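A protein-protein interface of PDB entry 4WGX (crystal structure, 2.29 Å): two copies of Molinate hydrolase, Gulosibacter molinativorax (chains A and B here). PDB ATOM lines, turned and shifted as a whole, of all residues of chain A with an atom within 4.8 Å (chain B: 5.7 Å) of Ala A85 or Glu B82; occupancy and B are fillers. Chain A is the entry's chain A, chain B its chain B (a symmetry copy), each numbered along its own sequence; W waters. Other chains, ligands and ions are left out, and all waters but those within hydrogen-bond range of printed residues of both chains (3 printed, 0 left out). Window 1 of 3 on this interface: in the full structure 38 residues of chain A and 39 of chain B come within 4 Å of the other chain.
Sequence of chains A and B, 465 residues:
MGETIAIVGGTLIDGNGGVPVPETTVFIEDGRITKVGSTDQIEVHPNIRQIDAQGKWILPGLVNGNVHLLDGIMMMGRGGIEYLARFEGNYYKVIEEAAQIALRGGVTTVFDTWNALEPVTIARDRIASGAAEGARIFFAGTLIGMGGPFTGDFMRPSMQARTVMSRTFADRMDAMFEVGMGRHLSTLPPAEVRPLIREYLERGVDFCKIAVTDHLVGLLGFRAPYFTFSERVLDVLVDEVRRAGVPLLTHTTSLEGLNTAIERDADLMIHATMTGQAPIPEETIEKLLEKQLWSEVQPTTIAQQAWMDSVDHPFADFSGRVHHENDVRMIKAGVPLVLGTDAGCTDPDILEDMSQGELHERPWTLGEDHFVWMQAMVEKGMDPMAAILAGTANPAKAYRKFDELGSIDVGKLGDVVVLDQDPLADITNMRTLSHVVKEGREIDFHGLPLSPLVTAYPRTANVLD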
ATOM      1  N   GLY A  80      14.836  14.069 -21.935  1.00  0.00           N
ATOM      2  CA  GLY A  80      14.011  14.250 -23.114  1.00  0.00           C
ATOM      3  C   GLY A  80      12.997  13.145 -23.381  1.00  0.00           C
ATOM      4  O   GLY A  80      11.817  13.411 -23.669  1.00  0.00           O
ATOM      5  N   ILE A  81      13.465  11.897 -23.301  1.00  0.00           N
ATOM      6  CA  ILE A  81      12.612  10.741 -23.542  1.00  0.00           C
ATOM      7  C   ILE A  81      11.453  10.699 -22.557  1.00  0.00           C
ATOM      8  O   ILE A  81      10.305  10.507 -22.941  1.00  0.00           O
ATOM      9  CB  ILE A  81      13.374   9.401 -23.430  1.00  0.00           C
ATOM     10  CG1 ILE A  81      14.507   9.333 -24.442  1.00  0.00           C
ATOM     11  CG2 ILE A  81      12.431   8.234 -23.673  1.00  0.00           C
ATOM     12  CD1 ILE A  81      15.514   8.237 -24.160  1.00  0.00           C
ATOM     13  N   GLU A  82      11.762  10.865 -21.282  1.00  0.00           N
ATOM     14  CA  GLU A  82      10.762  10.664 -20.253  1.00  0.00           C
ATOM     15  C   GLU A  82       9.698  11.766 -20.330  1.00  0.00           C
ATOM     16  O   GLU A  82       8.514  11.497 -20.223  1.00  0.00           O
ATOM     17  CB  GLU A  82      11.415  10.590 -18.866  1.00  0.00           C
ATOM     18  CG  GLU A  82      12.070  11.848 -18.353  1.00  0.00           C
ATOM     19  CD  GLU A  82      13.177  11.553 -17.344  1.00  0.00           C
ATOM     20  OE1 GLU A  82      14.228  11.018 -17.750  1.00  0.00           O
ATOM     21  OE2 GLU A  82      12.998  11.856 -16.150  1.00  0.00           O
ATOM     22  N   TYR A  83      10.145  12.994 -20.555  1.00  0.00           N
ATOM     23  CA  TYR A  83       9.275  14.161 -20.712  1.00  0.00           C
ATOM     24  C   TYR A  83       8.355  14.029 -21.937  1.00  0.00           C
ATOM     25  O   TYR A  83       7.105  14.113 -21.829  1.00  0.00           O
ATOM     26  CB  TYR A  83      10.179  15.390 -20.788  1.00  0.00           C
ATOM     27  CG  TYR A  83       9.586  16.748 -21.096  1.00  0.00           C
ATOM     28  CD1 TYR A  83       9.012  17.519 -20.098  1.00  0.00           C
ATOM     29  CD2 TYR A  83       9.685  17.297 -22.363  1.00  0.00           C
ATOM     30  CE1 TYR A  83       8.515  18.774 -20.364  1.00  0.00           C
ATOM     31  CE2 TYR A  83       9.191  18.558 -22.636  1.00  0.00           C
ATOM     32  CZ  TYR A  83       8.614  19.290 -21.631  1.00  0.00           C
ATOM     33  OH  TYR A  83       8.133  20.541 -21.895  1.00  0.00           O
ATOM     34  N   LEU A  84       8.952  13.766 -23.096  1.00  0.00           N
ATOM     35  CA  LEU A  84       8.142  13.631 -24.295  1.00  0.00           C
ATOM     36  C   LEU A  84       7.241  12.401 -24.268  1.00  0.00           C
ATOM     37  O   LEU A  84       6.142  12.436 -24.816  1.00  0.00           O
ATOM     38  CB  LEU A  84       9.021  13.605 -25.540  1.00  0.00           C
ATOM     39  CG  LEU A  84       9.752  14.916 -25.844  1.00  0.00           C
ATOM     40  CD1 LEU A  84      10.627  14.759 -27.064  1.00  0.00           C
ATOM     41  CD2 LEU A  84       8.785  16.066 -26.046  1.00  0.00           C
ATOM     42  N   ALA A  85       7.680  11.320 -23.640  1.00  0.00           N
ATOM     43  CA  ALA A  85       6.821  10.155 -23.541  1.00  0.00           C
ATOM     44  C   ALA A  85       5.701  10.393 -22.533  1.00  0.00           C
ATOM     45  O   ALA A  85       4.566  10.015 -22.763  1.00  0.00           O
ATOM     46  CB  ALA A  85       7.619   8.930 -23.165  1.00  0.00           C
ATOM     47  N   ARG A  86       6.034  11.032 -21.425  1.00  0.00           N
ATOM     48  CA  ARG A  86       5.065  11.291 -20.384  1.00  0.00           C
ATOM     49  C   ARG A  86       3.946  12.196 -20.884  1.00  0.00           C
ATOM     50  O   ARG A  86       2.788  11.968 -20.555  1.00  0.00           O
ATOM     51  CB  ARG A  86       5.721  11.930 -19.168  1.00  0.00           C
ATOM     52  CG  ARG A  86       4.818  11.978 -17.960  1.00  0.00           C
ATOM     53  CD  ARG A  86       5.453  12.691 -16.792  1.00  0.00           C
ATOM     54  NE  ARG A  86       6.718  12.089 -16.357  1.00  0.00           N
ATOM     55  CZ  ARG A  86       6.828  11.063 -15.518  1.00  0.00           C
ATOM     56  NH1 ARG A  86       5.750  10.483 -15.015  1.00  0.00           N
ATOM     57  NH2 ARG A  86       8.027  10.604 -15.182  1.00  0.00           N
ATOM     58  N   PHE A  87       4.282  13.219 -21.661  1.00  0.00           N
ATOM     59  CA  PHE A  87       3.239  14.165 -22.066  1.00  0.00           C
ATOM     60  C   PHE A  87       2.689  14.062 -23.486  1.00  0.00           C
ATOM     61  O   PHE A  87       1.947  14.934 -23.916  1.00  0.00           O
ATOM     62  CB  PHE A  87       3.755  15.566 -21.799  1.00  0.00           C
ATOM     63  CG  PHE A  87       4.044  15.791 -20.360  1.00  0.00           C
ATOM     64  CD1 PHE A  87       3.028  15.756 -19.432  1.00  0.00           C
ATOM     65  CD2 PHE A  87       5.329  15.959 -19.924  1.00  0.00           C
ATOM     66  CE1 PHE A  87       3.293  15.931 -18.106  1.00  0.00           C
ATOM     67  CE2 PHE A  87       5.596  16.127 -18.604  1.00  0.00           C
ATOM     68  CZ  PHE A  87       4.580  16.108 -17.691  1.00  0.00           C
ATOM     69  N   GLU A  88       2.996  12.987 -24.199  1.00  0.00           N
ATOM     70  CA  GLU A  88       2.374  12.770 -25.499  1.00  0.00           C
ATOM     71  C   GLU A  88       0.860  12.696 -25.320  1.00  0.00           C
ATOM     72  O   GLU A  88       0.375  12.032 -24.406  1.00  0.00           O
ATOM     73  CB  GLU A  88       2.904  11.496 -26.165  1.00  0.00           C
ATOM     74  CG  GLU A  88       2.477  11.361 -27.612  1.00  0.00           C
ATOM     75  CD  GLU A  88       3.291  10.359 -28.403  1.00  0.00           C
ATOM     76  OE1 GLU A  88       3.664   9.314 -27.846  1.00  0.00           O
ATOM     77  OE2 GLU A  88       3.545  10.614 -29.597  1.00  0.00           O
ATOM     78  N   VAL A 164      18.682   3.907 -26.425  1.00  0.00           N
ATOM     79  CA  VAL A 164      17.802   3.295 -25.428  1.00  0.00           C
ATOM     80  C   VAL A 164      16.303   3.588 -25.613  1.00  0.00           C
ATOM     81  O   VAL A 164      15.518   3.443 -24.681  1.00  0.00           O
ATOM     82  CB  VAL A 164      18.198   3.727 -24.007  1.00  0.00           C
ATOM     83  CG1 VAL A 164      19.581   3.218 -23.662  1.00  0.00           C
ATOM     84  CG2 VAL A 164      18.119   5.228 -23.857  1.00  0.00           C
ATOM     85  N   MET A 165      15.901   3.965 -26.817  1.00  0.00           N
ATOM     86  CA  MET A 165      14.493   4.212 -27.098  1.00  0.00           C
ATOM     87  C   MET A 165      14.105   3.545 -28.399  1.00  0.00           C
ATOM     88  O   MET A 165      14.960   3.159 -29.187  1.00  0.00           O
ATOM     89  CB  MET A 165      14.214   5.712 -27.153  1.00  0.00           C
ATOM     90  CG  MET A 165      14.871   6.418 -28.309  1.00  0.00           C
ATOM     91  SD  MET A 165      14.856   8.212 -28.168  1.00  0.00           S
ATOM     92  CE  MET A 165      13.100   8.526 -28.264  1.00  0.00           C
ATOM     93  N   SER A 166      12.809   3.373 -28.607  1.00  0.00           N
ATOM     94  CA  SER A 166      12.318   2.811 -29.854  1.00  0.00           C
ATOM     95  C   SER A 166      12.614   3.782 -30.978  1.00  0.00           C
ATOM     96  O   SER A 166      12.515   4.987 -30.793  1.00  0.00           O
ATOM     97  CB  SER A 166      10.818   2.539 -29.783  1.00  0.00           C
ATOM     98  OG  SER A 166      10.092   3.745 -29.675  1.00  0.00           O
ATOM     99  N   PHE A 169       9.218   5.793 -31.859  1.00  0.00           N
ATOM    100  CA  PHE A 169       8.963   6.952 -31.015  1.00  0.00           C
ATOM    101  C   PHE A 169       9.904   8.116 -31.338  1.00  0.00           C
ATOM    102  O   PHE A 169       9.477   9.274 -31.485  1.00  0.00           O
ATOM    103  CB  PHE A 169       9.097   6.587 -29.540  1.00  0.00           C
ATOM    104  CG  PHE A 169       8.799   7.719 -28.618  1.00  0.00           C
ATOM    105  CD1 PHE A 169       7.628   8.438 -28.757  1.00  0.00           C
ATOM    106  CD2 PHE A 169       9.682   8.076 -27.624  1.00  0.00           C
ATOM    107  CE1 PHE A 169       7.343   9.495 -27.920  1.00  0.00           C
ATOM    108  CE2 PHE A 169       9.401   9.125 -26.778  1.00  0.00           C
ATOM    109  CZ  PHE A 169       8.224   9.837 -26.926  1.00  0.00           C
ATOM    110  N   ARG B  78      15.851  -1.536 -25.595  1.00  0.00           N
ATOM    111  CA  ARG B  78      15.322  -0.217 -25.839  1.00  0.00           C
ATOM    112  C   ARG B  78      13.877  -0.166 -25.356  1.00  0.00           C
ATOM    113  O   ARG B  78      13.156  -1.151 -25.483  1.00  0.00           O
ATOM    114  CB  ARG B  78      15.445   0.103 -27.327  1.00  0.00           C
ATOM    115  CG  ARG B  78      16.893   0.126 -27.796  1.00  0.00           C
ATOM    116  CD  ARG B  78      17.056   0.416 -29.284  1.00  0.00           C
ATOM    117  NE  ARG B  78      15.882   0.057 -30.067  1.00  0.00           N
ATOM    118  CZ  ARG B  78      15.655  -1.147 -30.587  1.00  0.00           C
ATOM    119  NH1 ARG B  78      16.528  -2.136 -30.411  1.00  0.00           N
ATOM    120  NH2 ARG B  78      14.546  -1.367 -31.290  1.00  0.00           N
ATOM    121  N   GLY B  79      13.484   0.952 -24.749  1.00  0.00           N
ATOM    122  CA  GLY B  79      12.086   1.227 -24.456  1.00  0.00           C
ATOM    123  C   GLY B  79      11.683   1.379 -22.998  1.00  0.00           C
ATOM    124  O   GLY B  79      10.576   1.814 -22.713  1.00  0.00           O
ATOM    125  N   GLY B  80      12.567   1.037 -22.073  1.00  0.00           N
ATOM    126  CA  GLY B  80      12.258   1.120 -20.659  1.00  0.00           C
ATOM    127  C   GLY B  80      11.801   2.491 -20.186  1.00  0.00           C
ATOM    128  O   GLY B  80      10.784   2.620 -19.496  1.00  0.00           O
ATOM    129  N   ILE B  81      12.564   3.518 -20.545  1.00  0.00           N
ATOM    130  CA  ILE B  81      12.272   4.871 -20.089  1.00  0.00           C
ATOM    131  C   ILE B  81      10.915   5.344 -20.594  1.00  0.00           C
ATOM    132  O   ILE B  81      10.099   5.827 -19.822  1.00  0.00           O
ATOM    133  CB  ILE B  81      13.330   5.885 -20.548  1.00  0.00           C
ATOM    134  CG1 ILE B  81      14.711   5.537 -20.004  1.00  0.00           C
ATOM    135  CG2 ILE B  81      12.970   7.285 -20.058  1.00  0.00           C
ATOM    136  CD1 ILE B  81      15.832   6.237 -20.746  1.00  0.00           C
ATOM    137  N   GLU B  82      10.682   5.208 -21.893  1.00  0.00           N
ATOM    138  CA  GLU B  82       9.479   5.743 -22.510  1.00  0.00           C
ATOM    139  C   GLU B  82       8.246   5.017 -21.960  1.00  0.00           C
ATOM    140  O   GLU B  82       7.254   5.641 -21.592  1.00  0.00           O
ATOM    141  CB  GLU B  82       9.575   5.662 -24.048  1.00  0.00           C
ATOM    142  CG  GLU B  82       9.574   4.290 -24.692  1.00  0.00           C
ATOM    143  CD  GLU B  82      10.208   4.298 -26.097  1.00  0.00           C
ATOM    144  OE1 GLU B  82      11.447   4.392 -26.193  1.00  0.00           O
ATOM    145  OE2 GLU B  82       9.476   4.220 -27.108  1.00  0.00           O
ATOM    146  N   TYR B  83       8.349   3.703 -21.860  1.00  0.00           N
ATOM    147  CA  TYR B  83       7.296   2.868 -21.306  1.00  0.00           C
ATOM    148  C   TYR B  83       6.991   3.211 -19.861  1.00  0.00           C
ATOM    149  O   TYR B  83       5.842   3.437 -19.519  1.00  0.00           O
ATOM    150  CB  TYR B  83       7.707   1.412 -21.441  1.00  0.00           C
ATOM    151  CG  TYR B  83       6.787   0.360 -20.874  1.00  0.00           C
ATOM    152  CD1 TYR B  83       5.694  -0.109 -21.591  1.00  0.00           C
ATOM    153  CD2 TYR B  83       7.063  -0.234 -19.657  1.00  0.00           C
ATOM    154  CE1 TYR B  83       4.891  -1.106 -21.090  1.00  0.00           C
ATOM    155  CE2 TYR B  83       6.264  -1.233 -19.151  1.00  0.00           C
ATOM    156  CZ  TYR B  83       5.186  -1.666 -19.867  1.00  0.00           C
ATOM    157  OH  TYR B  83       4.410  -2.667 -19.345  1.00  0.00           O
ATOM    158  N   LEU B  84       8.004   3.269 -19.002  1.00  0.00           N
ATOM    159  CA  LEU B  84       7.724   3.583 -17.607  1.00  0.00           C
ATOM    160  C   LEU B  84       7.281   5.041 -17.397  1.00  0.00           C
ATOM    161  O   LEU B  84       6.504   5.317 -16.493  1.00  0.00           O
ATOM    162  CB  LEU B  84       8.934   3.275 -16.733  1.00  0.00           C
ATOM    163  CG  LEU B  84       9.247   1.784 -16.590  1.00  0.00           C
ATOM    164  CD1 LEU B  84      10.596   1.559 -15.908  1.00  0.00           C
ATOM    165  CD2 LEU B  84       8.132   1.064 -15.840  1.00  0.00           C
ATOM    166  N   ALA B  85       7.780   5.972 -18.207  1.00  0.00           N
ATOM    167  CA  ALA B  85       7.390   7.366 -18.054  1.00  0.00           C
ATOM    168  C   ALA B  85       5.955   7.577 -18.540  1.00  0.00           C
ATOM    169  O   ALA B  85       5.184   8.266 -17.909  1.00  0.00           O
ATOM    170  CB  ALA B  85       8.347   8.274 -18.806  1.00  0.00           C
ATOM    171  N   ARG B  86       5.607   6.948 -19.653  1.00  0.00           N
ATOM    172  CA  ARG B  86       4.289   7.091 -20.238  1.00  0.00           C
ATOM    173  C   ARG B  86       3.152   6.567 -19.351  1.00  0.00           C
ATOM    174  O   ARG B  86       2.048   7.107 -19.378  1.00  0.00           O
ATOM    175  CB  ARG B  86       4.256   6.383 -21.587  1.00  0.00           C
ATOM    176  CG  ARG B  86       3.037   6.686 -22.423  1.00  0.00           C
ATOM    177  CD  ARG B  86       3.000   5.831 -23.657  1.00  0.00           C
ATOM    178  NE  ARG B  86       4.103   6.104 -24.570  1.00  0.00           N
ATOM    179  CZ  ARG B  86       4.137   7.110 -25.440  1.00  0.00           C
ATOM    180  NH1 ARG B  86       3.139   7.975 -25.512  1.00  0.00           N
ATOM    181  NH2 ARG B  86       5.178   7.267 -26.232  1.00  0.00           N
ATOM    182  N   PHE B  87       3.418   5.534 -18.564  1.00  0.00           N
ATOM    183  CA  PHE B  87       2.351   4.879 -17.826  1.00  0.00           C
ATOM    184  C   PHE B  87       2.453   5.045 -16.312  1.00  0.00           C
ATOM    185  O   PHE B  87       1.690   4.443 -15.573  1.00  0.00           O
ATOM    186  CB  PHE B  87       2.302   3.398 -18.225  1.00  0.00           C
ATOM    187  CG  PHE B  87       1.985   3.195 -19.671  1.00  0.00           C
ATOM    188  CD1 PHE B  87       0.758   3.587 -20.186  1.00  0.00           C
ATOM    189  CD2 PHE B  87       2.914   2.656 -20.525  1.00  0.00           C
ATOM    190  CE1 PHE B  87       0.474   3.427 -21.510  1.00  0.00           C
ATOM    191  CE2 PHE B  87       2.637   2.502 -21.859  1.00  0.00           C
ATOM    192  CZ  PHE B  87       1.419   2.888 -22.354  1.00  0.00           C
ATOM    193  N   ASP B 347       5.283  -2.806 -25.646  1.00  0.00           N
ATOM    194  CA  ASP B 347       4.849  -1.521 -26.158  1.00  0.00           C
ATOM    195  C   ASP B 347       4.798  -1.526 -27.683  1.00  0.00           C
ATOM    196  O   ASP B 347       5.760  -1.928 -28.328  1.00  0.00           O
ATOM    197  CB  ASP B 347       5.781  -0.409 -25.681  1.00  0.00           C
ATOM    198  CG  ASP B 347       5.186   0.972 -25.874  1.00  0.00           C
ATOM    199  OD1 ASP B 347       5.336   1.538 -26.975  1.00  0.00           O
ATOM    200  OD2 ASP B 347       4.579   1.484 -24.915  1.00  0.00           O
ATOM    201  N   ASP B 349       5.183   0.775 -29.867  1.00  0.00           N
ATOM    202  CA  ASP B 349       6.274   1.508 -30.518  1.00  0.00           C
ATOM    203  C   ASP B 349       7.509   0.620 -30.667  1.00  0.00           C
ATOM    204  O   ASP B 349       8.255   0.743 -31.628  1.00  0.00           O
ATOM    205  CB  ASP B 349       6.660   2.765 -29.738  1.00  0.00           C
ATOM    206  CG  ASP B 349       5.768   3.955 -30.032  1.00  0.00           C
ATOM    207  OD1 ASP B 349       5.147   4.004 -31.105  1.00  0.00           O
ATOM    208  OD2 ASP B 349       5.721   4.863 -29.182  1.00  0.00           O
ATOM    209  N   ILE B 350       7.712  -0.280 -29.713  1.00  0.00           N
ATOM    210  CA  ILE B 350       8.818  -1.216 -29.785  1.00  0.00           C
ATOM    211  C   ILE B 350       8.495  -2.338 -30.764  1.00  0.00           C
ATOM    212  O   ILE B 350       9.350  -2.733 -31.543  1.00  0.00           O
ATOM    213  CB  ILE B 350       9.172  -1.780 -28.387  1.00  0.00           C
ATOM    214  CG1 ILE B 350       9.913  -0.715 -27.581  1.00  0.00           C
ATOM    215  CG2 ILE B 350      10.009  -3.066 -28.480  1.00  0.00           C
ATOM    216  CD1 ILE B 350      11.294  -0.372 -28.068  1.00  0.00           C
HETATM  217  O   HOH W   1      15.228   2.865 -21.996  1.00  0.00           O
HETATM  218  O   HOH W   2       1.568   9.755 -23.108  1.00  0.00           O
HETATM  219  O   HOH W   3      12.843   4.595 -23.935  1.00  0.00           O
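Among the printed residues, pairs that only touch across the chains: Met A165 with Glu B82 (3.2 Å), Ser A166 with Ile B350 (3.4 Å), Phe A169 with Glu B82 (3.4 Å), Glu A82 with Ala B85 (3.5 Å), Phe A169 with Arg B86 (3.5 Å), Ser A166 with Asp B349 (3.6 Å), Ala A85 with Glu B82 (3.7 Å), Ala A85 with Arg B86 (3.7 Å), Arg A86 with Ala B85 (3.7 Å), Ile A81 with Ile B81 (3.8 Å), Phe A169 with Asp B349 (3.8 Å), Glu A82 with Ile B81 (3.8 Å), Val A164 with Arg B78 (3.8 Å), Ile A81 with Glu B82 (3.9 Å) and Val A164 with Ile B81 (3.99 Å).
The side-chain carboxylate (OE1) of Glu A88 lies within salt-bridge range of the guanidinium group (NH1) of Arg B86. The backbone carbonyl oxygen (O) of Val A164 is in hydrogen-bond range of the backbone NH (N) of Gly B79, at 3.2 Å. The backbone carbonyl oxygen of Met A165 is in hydrogen-bond range of the guanidinium group of Arg B78, 3.4 Å away. The side-chain carboxylate (OE2) of Glu B82 lies within hydrogen-bond range of the side-chain hydroxyl (OG) of Ser A166, 2.7 Å away.
Printed residues of chain B within 4 Å of Glu A82: Ile B81 and Ala B85. Of the printed residues of chain B, Glu A88 touches Arg B86. Of the printed residues of chain A, Ile B81 touches Ile A81, Glu A82 and Val A164. Of the printed residues of chain A, Arg B86 touches Ala A85 (3.7 Å), Glu A88 (2.7 Å) and Phe A169 (3.5 Å). Asp B347 touches none of the printed residues of chain A. The nearest residue of chain B that does not touch Ala A85 is Ala B85 (4.5 Å).
Ile A81 touches its own counterpart, Ile B81. Ile A81 touches Glu B82, and with the chains exchanged Glu A82 touches Ile B81. Glu A82 touches Ala B85, and with the chains exchanged Ala A85 touches Glu B82. Ala A85 touches Arg B86, and with the chains exchanged Arg A86 touches Ala B85. 8 positions are printed for both chains. Of the 19 pairs that touch across the chains among the printed residues, 7 have their exchanged pair printed and touching as well.
OG of Ser A166 sits close to N of Phe A169, 3.1 Å away. NH2 of Arg B86 lies within salt-bridge range of OD2 of Asp B349, at 3.8 Å. The side-chain carboxylate (OD1) of Asp B347 lies within hydrogen-bond range of the backbone NH (N) of Asp B349 (3.0 Å).
Water W3 lies within hydrogen-bond range of the side-chain carboxylate of Glu B82 and the backbone carbonyl oxygen of Val A164. Water W1 lies within hydrogen-bond range of the backbone carbonyl oxygen (O) of Val A164 (2.8 Å), the backbone NH (N) of Ile B81 (3.1 Å) and the backbone NH (N) of Gly B80 (3.2 Å). Water W2 lies within hydrogen-bond range of O of Glu A88 (2.9 Å), O of Ala A85 (3.0 Å) and NH1 of Arg B86 (3.4 Å).
Printed residues of chain B that touch a printed residue of chain A: Arg B78, Gly B79, Ile B81, Glu B82, Ala B85, Arg B86, Asp B349 and Ile B350. Hydrophobic or aromatic side chains of chain B that line the printed part of chain A: Ile B81, Ala B85 and Ile B350. Of the 13 printed residues of chain A, 9 touch a printed residue of chain B. Printed residues of chain A that touch a printed residue of chain B: Ile A81, Glu A82, Ala A85, Arg A86, Glu A88, Val A164, Met A165, Ser A166 and Phe A169. Hydrophobic or aromatic side chains of chain A within 4 Å of the printed part of chain B: Ile A81, Ala A85, Val A164, Met A165 and Phe A169. Among the printed residues, Asp or Glu carboxylates within 4 Å of a Lys or Arg side-chain nitrogen of the other chain: Glu A88 with Arg B86 (2.7 Å).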
